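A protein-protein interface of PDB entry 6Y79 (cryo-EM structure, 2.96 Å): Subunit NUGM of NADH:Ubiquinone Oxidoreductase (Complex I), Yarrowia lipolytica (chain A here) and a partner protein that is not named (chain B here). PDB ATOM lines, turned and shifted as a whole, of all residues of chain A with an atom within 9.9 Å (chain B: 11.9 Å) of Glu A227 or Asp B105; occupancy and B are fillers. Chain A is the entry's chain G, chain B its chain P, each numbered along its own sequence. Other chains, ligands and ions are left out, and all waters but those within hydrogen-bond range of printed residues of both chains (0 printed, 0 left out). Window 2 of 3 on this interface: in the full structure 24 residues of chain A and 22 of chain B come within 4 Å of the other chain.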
ATOM      1  N   ARG A 223      -2.204   6.126  11.750  1.00  0.00           N
ATOM      2  CA  ARG A 223      -1.006   5.847  10.964  1.00  0.00           C
ATOM      3  C   ARG A 223      -1.421   5.392   9.576  1.00  0.00           C
ATOM      4  O   ARG A 223      -2.596   5.185   9.306  1.00  0.00           O
ATOM      5  CB  ARG A 223      -0.106   4.812  11.638  1.00  0.00           C
ATOM      6  CG  ARG A 223      -0.678   3.436  11.715  1.00  0.00           C
ATOM      7  CD  ARG A 223       0.348   2.485  12.271  1.00  0.00           C
ATOM      8  NE  ARG A 223      -0.213   1.157  12.461  1.00  0.00           N
ATOM      9  CZ  ARG A 223      -0.184   0.198  11.547  1.00  0.00           C
ATOM     10  NH1 ARG A 223      -0.733  -0.974  11.812  1.00  0.00           N
ATOM     11  NH2 ARG A 223       0.384   0.411  10.371  1.00  0.00           N
ATOM     12  N   TRP A 224      -0.445   5.270   8.682  1.00  0.00           N
ATOM     13  CA  TRP A 224      -0.682   4.695   7.360  1.00  0.00           C
ATOM     14  C   TRP A 224      -0.437   3.201   7.449  1.00  0.00           C
ATOM     15  O   TRP A 224       0.689   2.765   7.707  1.00  0.00           O
ATOM     16  CB  TRP A 224       0.217   5.317   6.298  1.00  0.00           C
ATOM     17  CG  TRP A 224       0.019   4.792   4.907  1.00  0.00           C
ATOM     18  CD1 TRP A 224       0.783   3.870   4.258  1.00  0.00           C
ATOM     19  CD2 TRP A 224      -0.995   5.186   3.987  1.00  0.00           C
ATOM     20  NE1 TRP A 224       0.297   3.658   2.993  1.00  0.00           N
ATOM     21  CE2 TRP A 224      -0.798   4.456   2.804  1.00  0.00           C
ATOM     22  CE3 TRP A 224      -2.055   6.084   4.050  1.00  0.00           C
ATOM     23  CZ2 TRP A 224      -1.622   4.599   1.699  1.00  0.00           C
ATOM     24  CZ3 TRP A 224      -2.876   6.212   2.970  1.00  0.00           C
ATOM     25  CH2 TRP A 224      -2.653   5.486   1.800  1.00  0.00           C
ATOM     26  N   ASP A 225      -1.492   2.421   7.268  1.00  0.00           N
ATOM     27  CA  ASP A 225      -1.334   0.991   7.083  1.00  0.00           C
ATOM     28  C   ASP A 225      -0.920   0.730   5.642  1.00  0.00           C
ATOM     29  O   ASP A 225      -1.543   1.245   4.711  1.00  0.00           O
ATOM     30  CB  ASP A 225      -2.646   0.292   7.405  1.00  0.00           C
ATOM     31  CG  ASP A 225      -2.532  -1.202   7.378  1.00  0.00           C
ATOM     32  OD1 ASP A 225      -2.047  -1.793   8.363  1.00  0.00           O
ATOM     33  OD2 ASP A 225      -2.925  -1.785   6.358  1.00  0.00           O
ATOM     34  N   GLU A 226       0.157  -0.035   5.447  1.00  0.00           N
ATOM     35  CA  GLU A 226       0.565  -0.317   4.075  1.00  0.00           C
ATOM     36  C   GLU A 226      -0.269  -1.447   3.487  1.00  0.00           C
ATOM     37  O   GLU A 226      -0.535  -1.465   2.277  1.00  0.00           O
ATOM     38  CB  GLU A 226       2.059  -0.650   3.993  1.00  0.00           C
ATOM     39  CG  GLU A 226       2.561  -0.689   2.541  1.00  0.00           C
ATOM     40  CD  GLU A 226       4.026  -1.023   2.374  1.00  0.00           C
ATOM     41  OE1 GLU A 226       4.733  -1.174   3.374  1.00  0.00           O
ATOM     42  OE2 GLU A 226       4.475  -1.190   1.220  1.00  0.00           O
ATOM     43  N   GLU A 227      -0.726  -2.371   4.337  1.00  0.00           N
ATOM     44  CA  GLU A 227      -1.538  -3.495   3.882  1.00  0.00           C
ATOM     45  C   GLU A 227      -2.872  -3.021   3.305  1.00  0.00           C
ATOM     46  O   GLU A 227      -3.220  -3.357   2.169  1.00  0.00           O
ATOM     47  CB  GLU A 227      -1.744  -4.482   5.035  1.00  0.00           C
ATOM     48  CG  GLU A 227      -2.953  -5.379   4.896  1.00  0.00           C
ATOM     49  CD  GLU A 227      -3.182  -6.238   6.118  1.00  0.00           C
ATOM     50  OE1 GLU A 227      -2.584  -5.943   7.172  1.00  0.00           O
ATOM     51  OE2 GLU A 227      -3.956  -7.212   6.024  1.00  0.00           O
ATOM     52  N   LYS A 228      -3.611  -2.196   4.046  1.00  0.00           N
ATOM     53  CA  LYS A 228      -4.896  -1.723   3.545  1.00  0.00           C
ATOM     54  C   LYS A 228      -4.789  -0.525   2.615  1.00  0.00           C
ATOM     55  O   LYS A 228      -5.804  -0.165   2.007  1.00  0.00           O
ATOM     56  CB  LYS A 228      -5.825  -1.360   4.697  1.00  0.00           C
ATOM     57  CG  LYS A 228      -6.030  -2.474   5.676  1.00  0.00           C
ATOM     58  CD  LYS A 228      -6.931  -2.043   6.790  1.00  0.00           C
ATOM     59  CE  LYS A 228      -6.700  -2.909   8.003  1.00  0.00           C
ATOM     60  NZ  LYS A 228      -7.633  -2.547   9.095  1.00  0.00           N
ATOM     61  N   ARG A 229      -3.603   0.087   2.505  1.00  0.00           N
ATOM     62  CA  ARG A 229      -3.351   1.279   1.681  1.00  0.00           C
ATOM     63  C   ARG A 229      -4.283   2.434   2.051  1.00  0.00           C
ATOM     64  O   ARG A 229      -4.800   3.144   1.186  1.00  0.00           O
ATOM     65  CB  ARG A 229      -3.434   0.962   0.184  1.00  0.00           C
ATOM     66  CG  ARG A 229      -2.428  -0.079  -0.291  1.00  0.00           C
ATOM     67  CD  ARG A 229      -1.034   0.507  -0.405  1.00  0.00           C
ATOM     68  NE  ARG A 229      -0.057  -0.480  -0.854  1.00  0.00           N
ATOM     69  CZ  ARG A 229       0.281  -0.668  -2.125  1.00  0.00           C
ATOM     70  NH1 ARG A 229      -0.278   0.065  -3.076  1.00  0.00           N
ATOM     71  NH2 ARG A 229       1.180  -1.587  -2.446  1.00  0.00           N
ATOM     72  N   ARG A 230      -4.504   2.613   3.350  1.00  0.00           N
ATOM     73  CA  ARG A 230      -5.236   3.755   3.877  1.00  0.00           C
ATOM     74  C   ARG A 230      -4.660   4.085   5.245  1.00  0.00           C
ATOM     75  O   ARG A 230      -3.828   3.346   5.780  1.00  0.00           O
ATOM     76  CB  ARG A 230      -6.737   3.477   3.961  1.00  0.00           C
ATOM     77  CG  ARG A 230      -7.116   2.386   4.937  1.00  0.00           C
ATOM     78  CD  ARG A 230      -8.619   2.222   4.984  1.00  0.00           C
ATOM     79  NE  ARG A 230      -9.023   1.090   5.810  1.00  0.00           N
ATOM     80  CZ  ARG A 230      -9.315   1.182   7.101  1.00  0.00           C
ATOM     81  NH1 ARG A 230      -9.672   0.105   7.778  1.00  0.00           N
ATOM     82  NH2 ARG A 230      -9.248   2.354   7.714  1.00  0.00           N
ATOM     83  N   VAL A 231      -5.090   5.212   5.814  1.00  0.00           N
ATOM     84  CA  VAL A 231      -4.760   5.464   7.210  1.00  0.00           C
ATOM     85  C   VAL A 231      -5.731   4.679   8.082  1.00  0.00           C
ATOM     86  O   VAL A 231      -6.915   4.524   7.764  1.00  0.00           O
ATOM     87  CB  VAL A 231      -4.738   6.975   7.551  1.00  0.00           C
ATOM     88  CG1 VAL A 231      -3.876   7.748   6.587  1.00  0.00           C
ATOM     89  CG2 VAL A 231      -6.093   7.603   7.626  1.00  0.00           C
ATOM     90  N   VAL A 232      -5.201   4.097   9.140  1.00  0.00           N
ATOM     91  CA  VAL A 232      -5.993   3.380  10.119  1.00  0.00           C
ATOM     92  C   VAL A 232      -5.945   4.153  11.421  1.00  0.00           C
ATOM     93  O   VAL A 232      -4.988   4.883  11.715  1.00  0.00           O
ATOM     94  CB  VAL A 232      -5.514   1.932  10.334  1.00  0.00           C
ATOM     95  CG1 VAL A 232      -5.834   1.094   9.120  1.00  0.00           C
ATOM     96  CG2 VAL A 232      -4.038   1.900  10.647  1.00  0.00           C
ATOM     97  N   GLU A 234      -6.129   3.690  15.426  1.00  0.00           N
ATOM     98  CA  GLU A 234      -5.770   2.658  16.380  1.00  0.00           C
ATOM     99  C   GLU A 234      -5.915   3.199  17.789  1.00  0.00           C
ATOM    100  O   GLU A 234      -5.991   4.415  17.980  1.00  0.00           O
ATOM    101  CB  GLU A 234      -4.329   2.198  16.136  1.00  0.00           C
ATOM    102  CG  GLU A 234      -4.211   1.258  14.973  1.00  0.00           C
ATOM    103  CD  GLU A 234      -2.809   0.754  14.790  1.00  0.00           C
ATOM    104  OE1 GLU A 234      -2.304   0.847  13.659  1.00  0.00           O
ATOM    105  OE2 GLU A 234      -2.212   0.266  15.769  1.00  0.00           O
ATOM    106  N   GLN B  46     -14.907  -2.317  -0.625  1.00  0.00           N
ATOM    107  CA  GLN B  46     -14.524  -3.627  -1.148  1.00  0.00           C
ATOM    108  C   GLN B  46     -15.713  -4.552  -1.336  1.00  0.00           C
ATOM    109  O   GLN B  46     -15.796  -5.269  -2.338  1.00  0.00           O
ATOM    110  CB  GLN B  46     -13.560  -4.319  -0.189  1.00  0.00           C
ATOM    111  CG  GLN B  46     -12.168  -3.758  -0.120  1.00  0.00           C
ATOM    112  CD  GLN B  46     -11.484  -4.129   1.184  1.00  0.00           C
ATOM    113  OE1 GLN B  46     -11.199  -5.302   1.437  1.00  0.00           O
ATOM    114  NE2 GLN B  46     -11.226  -3.131   2.022  1.00  0.00           N
ATOM    115  N   PHE B  47     -16.617  -4.542  -0.381  1.00  0.00           N
ATOM    116  CA  PHE B  47     -17.667  -5.505  -0.122  1.00  0.00           C
ATOM    117  C   PHE B  47     -18.962  -5.043  -0.795  1.00  0.00           C
ATOM    118  O   PHE B  47     -18.949  -4.125  -1.623  1.00  0.00           O
ATOM    119  CB  PHE B  47     -17.793  -5.653   1.397  1.00  0.00           C
ATOM    120  CG  PHE B  47     -18.099  -4.359   2.100  1.00  0.00           C
ATOM    121  CD1 PHE B  47     -17.092  -3.505   2.523  1.00  0.00           C
ATOM    122  CD2 PHE B  47     -19.403  -3.990   2.324  1.00  0.00           C
ATOM    123  CE1 PHE B  47     -17.391  -2.321   3.153  1.00  0.00           C
ATOM    124  CE2 PHE B  47     -19.702  -2.820   2.952  1.00  0.00           C
ATOM    125  CZ  PHE B  47     -18.702  -1.979   3.362  1.00  0.00           C
ATOM    126  N   THR B  51     -23.728  -5.527   3.772  1.00  0.00           N
ATOM    127  CA  THR B  51     -22.882  -5.391   4.952  1.00  0.00           C
ATOM    128  C   THR B  51     -22.987  -3.985   5.547  1.00  0.00           C
ATOM    129  O   THR B  51     -22.950  -3.827   6.774  1.00  0.00           O
ATOM    130  CB  THR B  51     -21.442  -5.755   4.606  1.00  0.00           C
ATOM    131  OG1 THR B  51     -21.433  -6.998   3.897  1.00  0.00           O
ATOM    132  CG2 THR B  51     -20.619  -5.924   5.859  1.00  0.00           C
ATOM    133  N   GLN B  93     -13.147   7.995   3.159  1.00  0.00           N
ATOM    134  CA  GLN B  93     -13.189   6.538   3.213  1.00  0.00           C
ATOM    135  C   GLN B  93     -12.436   5.999   4.417  1.00  0.00           C
ATOM    136  O   GLN B  93     -12.840   4.989   5.003  1.00  0.00           O
ATOM    137  CB  GLN B  93     -12.611   5.954   1.925  1.00  0.00           C
ATOM    138  CG  GLN B  93     -12.639   4.439   1.870  1.00  0.00           C
ATOM    139  CD  GLN B  93     -11.618   3.857   0.933  1.00  0.00           C
ATOM    140  OE1 GLN B  93     -11.078   4.550   0.076  1.00  0.00           O
ATOM    141  NE2 GLN B  93     -11.356   2.563   1.078  1.00  0.00           N
ATOM    142  N   LEU B  97     -14.537   3.780   7.049  1.00  0.00           N
ATOM    143  CA  LEU B  97     -14.097   2.448   7.432  1.00  0.00           C
ATOM    144  C   LEU B  97     -13.629   2.371   8.876  1.00  0.00           C
ATOM    145  O   LEU B  97     -13.018   1.370   9.260  1.00  0.00           O
ATOM    146  CB  LEU B  97     -12.984   1.969   6.502  1.00  0.00           C
ATOM    147  CG  LEU B  97     -13.403   1.723   5.054  1.00  0.00           C
ATOM    148  CD1 LEU B  97     -12.214   1.299   4.226  1.00  0.00           C
ATOM    149  CD2 LEU B  97     -14.502   0.691   4.983  1.00  0.00           C
ATOM    150  N   LYS B  98     -13.875   3.414   9.674  1.00  0.00           N
ATOM    151  CA  LYS B  98     -13.793   3.275  11.123  1.00  0.00           C
ATOM    152  C   LYS B  98     -14.826   2.280  11.624  1.00  0.00           C
ATOM    153  O   LYS B  98     -14.573   1.540  12.580  1.00  0.00           O
ATOM    154  CB  LYS B  98     -14.019   4.620  11.804  1.00  0.00           C
ATOM    155  CG  LYS B  98     -12.864   5.575  11.804  1.00  0.00           C
ATOM    156  CD  LYS B  98     -13.292   6.842  12.502  1.00  0.00           C
ATOM    157  CE  LYS B  98     -13.508   6.586  13.973  1.00  0.00           C
ATOM    158  NZ  LYS B  98     -12.241   6.335  14.704  1.00  0.00           N
ATOM    159  N   TYR B  99     -15.995   2.238  10.967  1.00  0.00           N
ATOM    160  CA  TYR B  99     -17.128   1.416  11.394  1.00  0.00           C
ATOM    161  C   TYR B  99     -16.894  -0.053  11.182  1.00  0.00           C
ATOM    162  O   TYR B  99     -17.638  -0.871  11.727  1.00  0.00           O
ATOM    163  CB  TYR B  99     -18.406   1.806  10.646  1.00  0.00           C
ATOM    164  CG  TYR B  99     -18.828   3.186  11.034  1.00  0.00           C
ATOM    165  CD1 TYR B  99     -18.464   3.663  12.256  1.00  0.00           C
ATOM    166  CD2 TYR B  99     -19.526   4.016  10.186  1.00  0.00           C
ATOM    167  CE1 TYR B  99     -18.741   4.887  12.667  1.00  0.00           C
ATOM    168  CE2 TYR B  99     -19.863   5.304  10.582  1.00  0.00           C
ATOM    169  CZ  TYR B  99     -19.445   5.709  11.863  1.00  0.00           C
ATOM    170  OH  TYR B  99     -19.658   6.920  12.435  1.00  0.00           O
ATOM    171  N   PHE B 100     -15.884  -0.402  10.399  1.00  0.00           N
ATOM    172  CA  PHE B 100     -15.616  -1.779  10.016  1.00  0.00           C
ATOM    173  C   PHE B 100     -14.209  -2.195  10.421  1.00  0.00           C
ATOM    174  O   PHE B 100     -13.395  -2.527   9.549  1.00  0.00           O
ATOM    175  CB  PHE B 100     -15.773  -1.917   8.506  1.00  0.00           C
ATOM    176  CG  PHE B 100     -17.141  -1.635   8.014  1.00  0.00           C
ATOM    177  CD1 PHE B 100     -18.231  -2.228   8.607  1.00  0.00           C
ATOM    178  CD2 PHE B 100     -17.341  -0.777   6.955  1.00  0.00           C
ATOM    179  CE1 PHE B 100     -19.490  -1.983   8.142  1.00  0.00           C
ATOM    180  CE2 PHE B 100     -18.608  -0.522   6.497  1.00  0.00           C
ATOM    181  CZ  PHE B 100     -19.680  -1.137   7.088  1.00  0.00           C
ATOM    182  N   PRO B 101     -13.883  -2.230  11.737  1.00  0.00           N
ATOM    183  CA  PRO B 101     -12.512  -2.622  12.104  1.00  0.00           C
ATOM    184  C   PRO B 101     -12.300  -4.123  11.967  1.00  0.00           C
ATOM    185  O   PRO B 101     -11.180  -4.625  11.864  1.00  0.00           O
ATOM    186  CB  PRO B 101     -12.394  -2.150  13.558  1.00  0.00           C
ATOM    187  CG  PRO B 101     -13.782  -2.240  14.085  1.00  0.00           C
ATOM    188  CD  PRO B 101     -14.723  -2.026  12.938  1.00  0.00           C
ATOM    189  N   GLU B 102     -13.418  -4.828  11.930  1.00  0.00           N
ATOM    190  CA  GLU B 102     -13.539  -6.266  12.036  1.00  0.00           C
ATOM    191  C   GLU B 102     -13.380  -6.957  10.692  1.00  0.00           C
ATOM    192  O   GLU B 102     -13.101  -8.152  10.645  1.00  0.00           O
ATOM    193  CB  GLU B 102     -14.918  -6.581  12.594  1.00  0.00           C
ATOM    194  CG  GLU B 102     -15.955  -5.798  11.794  1.00  0.00           C
ATOM    195  CD  GLU B 102     -17.328  -5.727  12.377  1.00  0.00           C
ATOM    196  OE1 GLU B 102     -18.258  -5.437  11.587  1.00  0.00           O
ATOM    197  OE2 GLU B 102     -17.505  -5.942  13.595  1.00  0.00           O
ATOM    198  N   GLU B 103     -13.578  -6.221   9.606  1.00  0.00           N
ATOM    199  CA  GLU B 103     -13.918  -6.764   8.301  1.00  0.00           C
ATOM    200  C   GLU B 103     -12.732  -6.696   7.355  1.00  0.00           C
ATOM    201  O   GLU B 103     -12.585  -7.557   6.476  1.00  0.00           O
ATOM    202  CB  GLU B 103     -15.116  -5.973   7.787  1.00  0.00           C
ATOM    203  CG  GLU B 103     -15.512  -6.186   6.370  1.00  0.00           C
ATOM    204  CD  GLU B 103     -16.290  -5.003   5.865  1.00  0.00           C
ATOM    205  OE1 GLU B 103     -15.676  -4.164   5.184  1.00  0.00           O
ATOM    206  OE2 GLU B 103     -17.499  -4.897   6.158  1.00  0.00           O
ATOM    207  N   ASP B 104     -11.875  -5.687   7.574  1.00  0.00           N
ATOM    208  CA  ASP B 104     -10.794  -5.350   6.665  1.00  0.00           C
ATOM    209  C   ASP B 104      -9.782  -6.475   6.576  1.00  0.00           C
ATOM    210  O   ASP B 104      -9.344  -6.837   5.480  1.00  0.00           O
ATOM    211  CB  ASP B 104     -10.089  -4.095   7.150  1.00  0.00           C
ATOM    212  CG  ASP B 104     -10.995  -2.885   7.194  1.00  0.00           C
ATOM    213  OD1 ASP B 104     -11.879  -2.744   6.330  1.00  0.00           O
ATOM    214  OD2 ASP B 104     -10.810  -2.087   8.132  1.00  0.00           O
ATOM    215  N   ASP B 105      -9.380  -7.021   7.715  1.00  0.00           N
ATOM    216  CA  ASP B 105      -8.323  -8.016   7.736  1.00  0.00           C
ATOM    217  C   ASP B 105      -8.527  -8.935   8.927  1.00  0.00           C
ATOM    218  O   ASP B 105      -9.299  -8.615   9.834  1.00  0.00           O
ATOM    219  CB  ASP B 105      -6.938  -7.341   7.773  1.00  0.00           C
ATOM    220  CG  ASP B 105      -6.708  -6.440   9.008  1.00  0.00           C
ATOM    221  OD1 ASP B 105      -7.592  -6.255   9.867  1.00  0.00           O
ATOM    222  OD2 ASP B 105      -5.588  -5.892   9.113  1.00  0.00           O
ATOM    223  N   ILE B 106      -7.843 -10.069   8.918  1.00  0.00           N
ATOM    224  CA  ILE B 106      -7.637 -10.800  10.158  1.00  0.00           C
ATOM    225  C   ILE B 106      -6.345 -10.285  10.789  1.00  0.00           C
ATOM    226  O   ILE B 106      -5.327 -10.115  10.108  1.00  0.00           O
ATOM    227  CB  ILE B 106      -7.631 -12.323   9.924  1.00  0.00           C
ATOM    228  CG1 ILE B 106      -7.629 -13.075  11.256  1.00  0.00           C
ATOM    229  CG2 ILE B 106      -6.558 -12.796   8.934  1.00  0.00           C
ATOM    230  CD1 ILE B 106      -8.963 -13.019  11.957  1.00  0.00           C
ATOM    231  N   GLN B 107      -6.408  -9.927  12.073  1.00  0.00           N
ATOM    232  CA  GLN B 107      -5.275  -9.226  12.669  1.00  0.00           C
ATOM    233  C   GLN B 107      -4.135 -10.173  13.024  1.00  0.00           C
ATOM    234  O   GLN B 107      -3.006  -9.713  13.225  1.00  0.00           O
ATOM    235  CB  GLN B 107      -5.735  -8.423  13.885  1.00  0.00           C
ATOM    236  CG  GLN B 107      -6.741  -7.313  13.540  1.00  0.00           C
ATOM    237  CD  GLN B 107      -6.659  -6.108  14.472  1.00  0.00           C
ATOM    238  OE1 GLN B 107      -6.475  -6.252  15.680  1.00  0.00           O
ATOM    239  NE2 GLN B 107      -6.806  -4.911  13.908  1.00  0.00           N
ATOM    240  N   GLY B 108      -4.391 -11.471  13.085  1.00  0.00           N
ATOM    241  CA  GLY B 108      -3.323 -12.449  13.146  1.00  0.00           C
ATOM    242  C   GLY B 108      -3.752 -13.688  13.904  1.00  0.00           C
ATOM    243  O   GLY B 108      -4.933 -13.929  14.129  1.00  0.00           O
ATOM    244  N   ARG B 109      -2.753 -14.475  14.298  1.00  0.00           N
ATOM    245  CA  ARG B 109      -2.991 -15.648  15.122  1.00  0.00           C
ATOM    246  C   ARG B 109      -3.293 -15.273  16.553  1.00  0.00           C
ATOM    247  O   ARG B 109      -3.386 -14.097  16.918  1.00  0.00           O
ATOM    248  CB  ARG B 109      -1.776 -16.547  15.207  1.00  0.00           C
ATOM    249  CG  ARG B 109      -1.338 -17.216  13.962  1.00  0.00           C
ATOM    250  CD  ARG B 109      -0.009 -17.907  14.286  1.00  0.00           C
ATOM    251  NE  ARG B 109      -0.121 -19.154  14.972  1.00  0.00           N
ATOM    252  CZ  ARG B 109      -0.298 -20.326  14.381  1.00  0.00           C
ATOM    253  NH1 ARG B 109      -0.351 -21.467  15.076  1.00  0.00           N
ATOM    254  NH2 ARG B 109      -0.438 -20.349  13.081  1.00  0.00           N
ATOM    255  N   GLN B 111      -5.428 -15.517  19.218  1.00  0.00           N
ATOM    256  CA  GLN B 111      -6.449 -14.714  19.860  1.00  0.00           C
ATOM    257  C   GLN B 111      -6.649 -15.232  21.274  1.00  0.00           C
ATOM    258  O   GLN B 111      -7.029 -16.396  21.447  1.00  0.00           O
ATOM    259  CB  GLN B 111      -7.752 -14.777  19.074  1.00  0.00           C
ATOM    260  CG  GLN B 111      -7.650 -14.229  17.660  1.00  0.00           C
ATOM    261  CD  GLN B 111      -7.528 -12.717  17.625  1.00  0.00           C
ATOM    262  OE1 GLN B 111      -7.996 -12.024  18.529  1.00  0.00           O
ATOM    263  NE2 GLN B 111      -6.902 -12.199  16.576  1.00  0.00           N
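The side-chain carboxylate (OD2) of Asp B104 lies within salt-bridge range of the side-chain amino group (NZ) of Lys A228, at 3.4 Å. The side-chain carboxylate (OD2) of Asp B104 is in salt-bridge range of the guanidinium group (NH1) of Arg A230. OD1 of Asp B105 lies within salt-bridge range of NZ of Lys A228, 3.8 Å away.
The side-chain carboxylate (OD2) of Asp A225 is in hydrogen-bond range of the backbone NH (N) of Glu A227, at 3.0 Å. The side-chain carboxylate of Asp A225 is in hydrogen-bond range of the backbone NH of Lys A228 (2.4 Å). The backbone NH (N) of Asp A225 sits at hydrogen-bond distance from the backbone carbonyl oxygen (O) of Arg A230 (2.9 Å).
Among the printed residues, pairs that only touch across the chains: Glu A227 with Asp B105 (3.5 Å) and Arg A230 with Leu B97 (3.6 Å).
Glu A227 touches just one residue of chain B: Asp B105 (3.5 Å). Of chain A, only Glu A227 (3.5 Å) and Lys A228 (3.4 Å) come within 4 Å of Asp B105. No residue of chain B comes within 4 Å of Asp A225. No residue of chain B comes within 4 Å of Glu A226. Of chain B, only Asp B104 (3.4 Å) and Asp B105 (3.4 Å) come within 4 Å of Lys A228. No residue of chain A comes within 4 Å of Ile B106. Printed residues of chain B within 4 Å of Arg A230: Leu B97 and Asp B104. Printed residues of chain A within 4 Å of Leu B97: Arg A230 (3.6 Å). The nearest residue of chain B that does not touch Glu A227 is Ile B106 (5.2 Å). The nearest residue of chain A that does not touch Asp B105 is Asp A225 (5.5 Å). The nearest printed residue of chain B that does not touch Arg A230 is Gln B93 (4.8 Å).
Hydrophobic or aromatic side chains of chain B within 4 Å of the printed part of chain A: Leu B97. Among the printed residues, 5 pairs touch across the chains.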
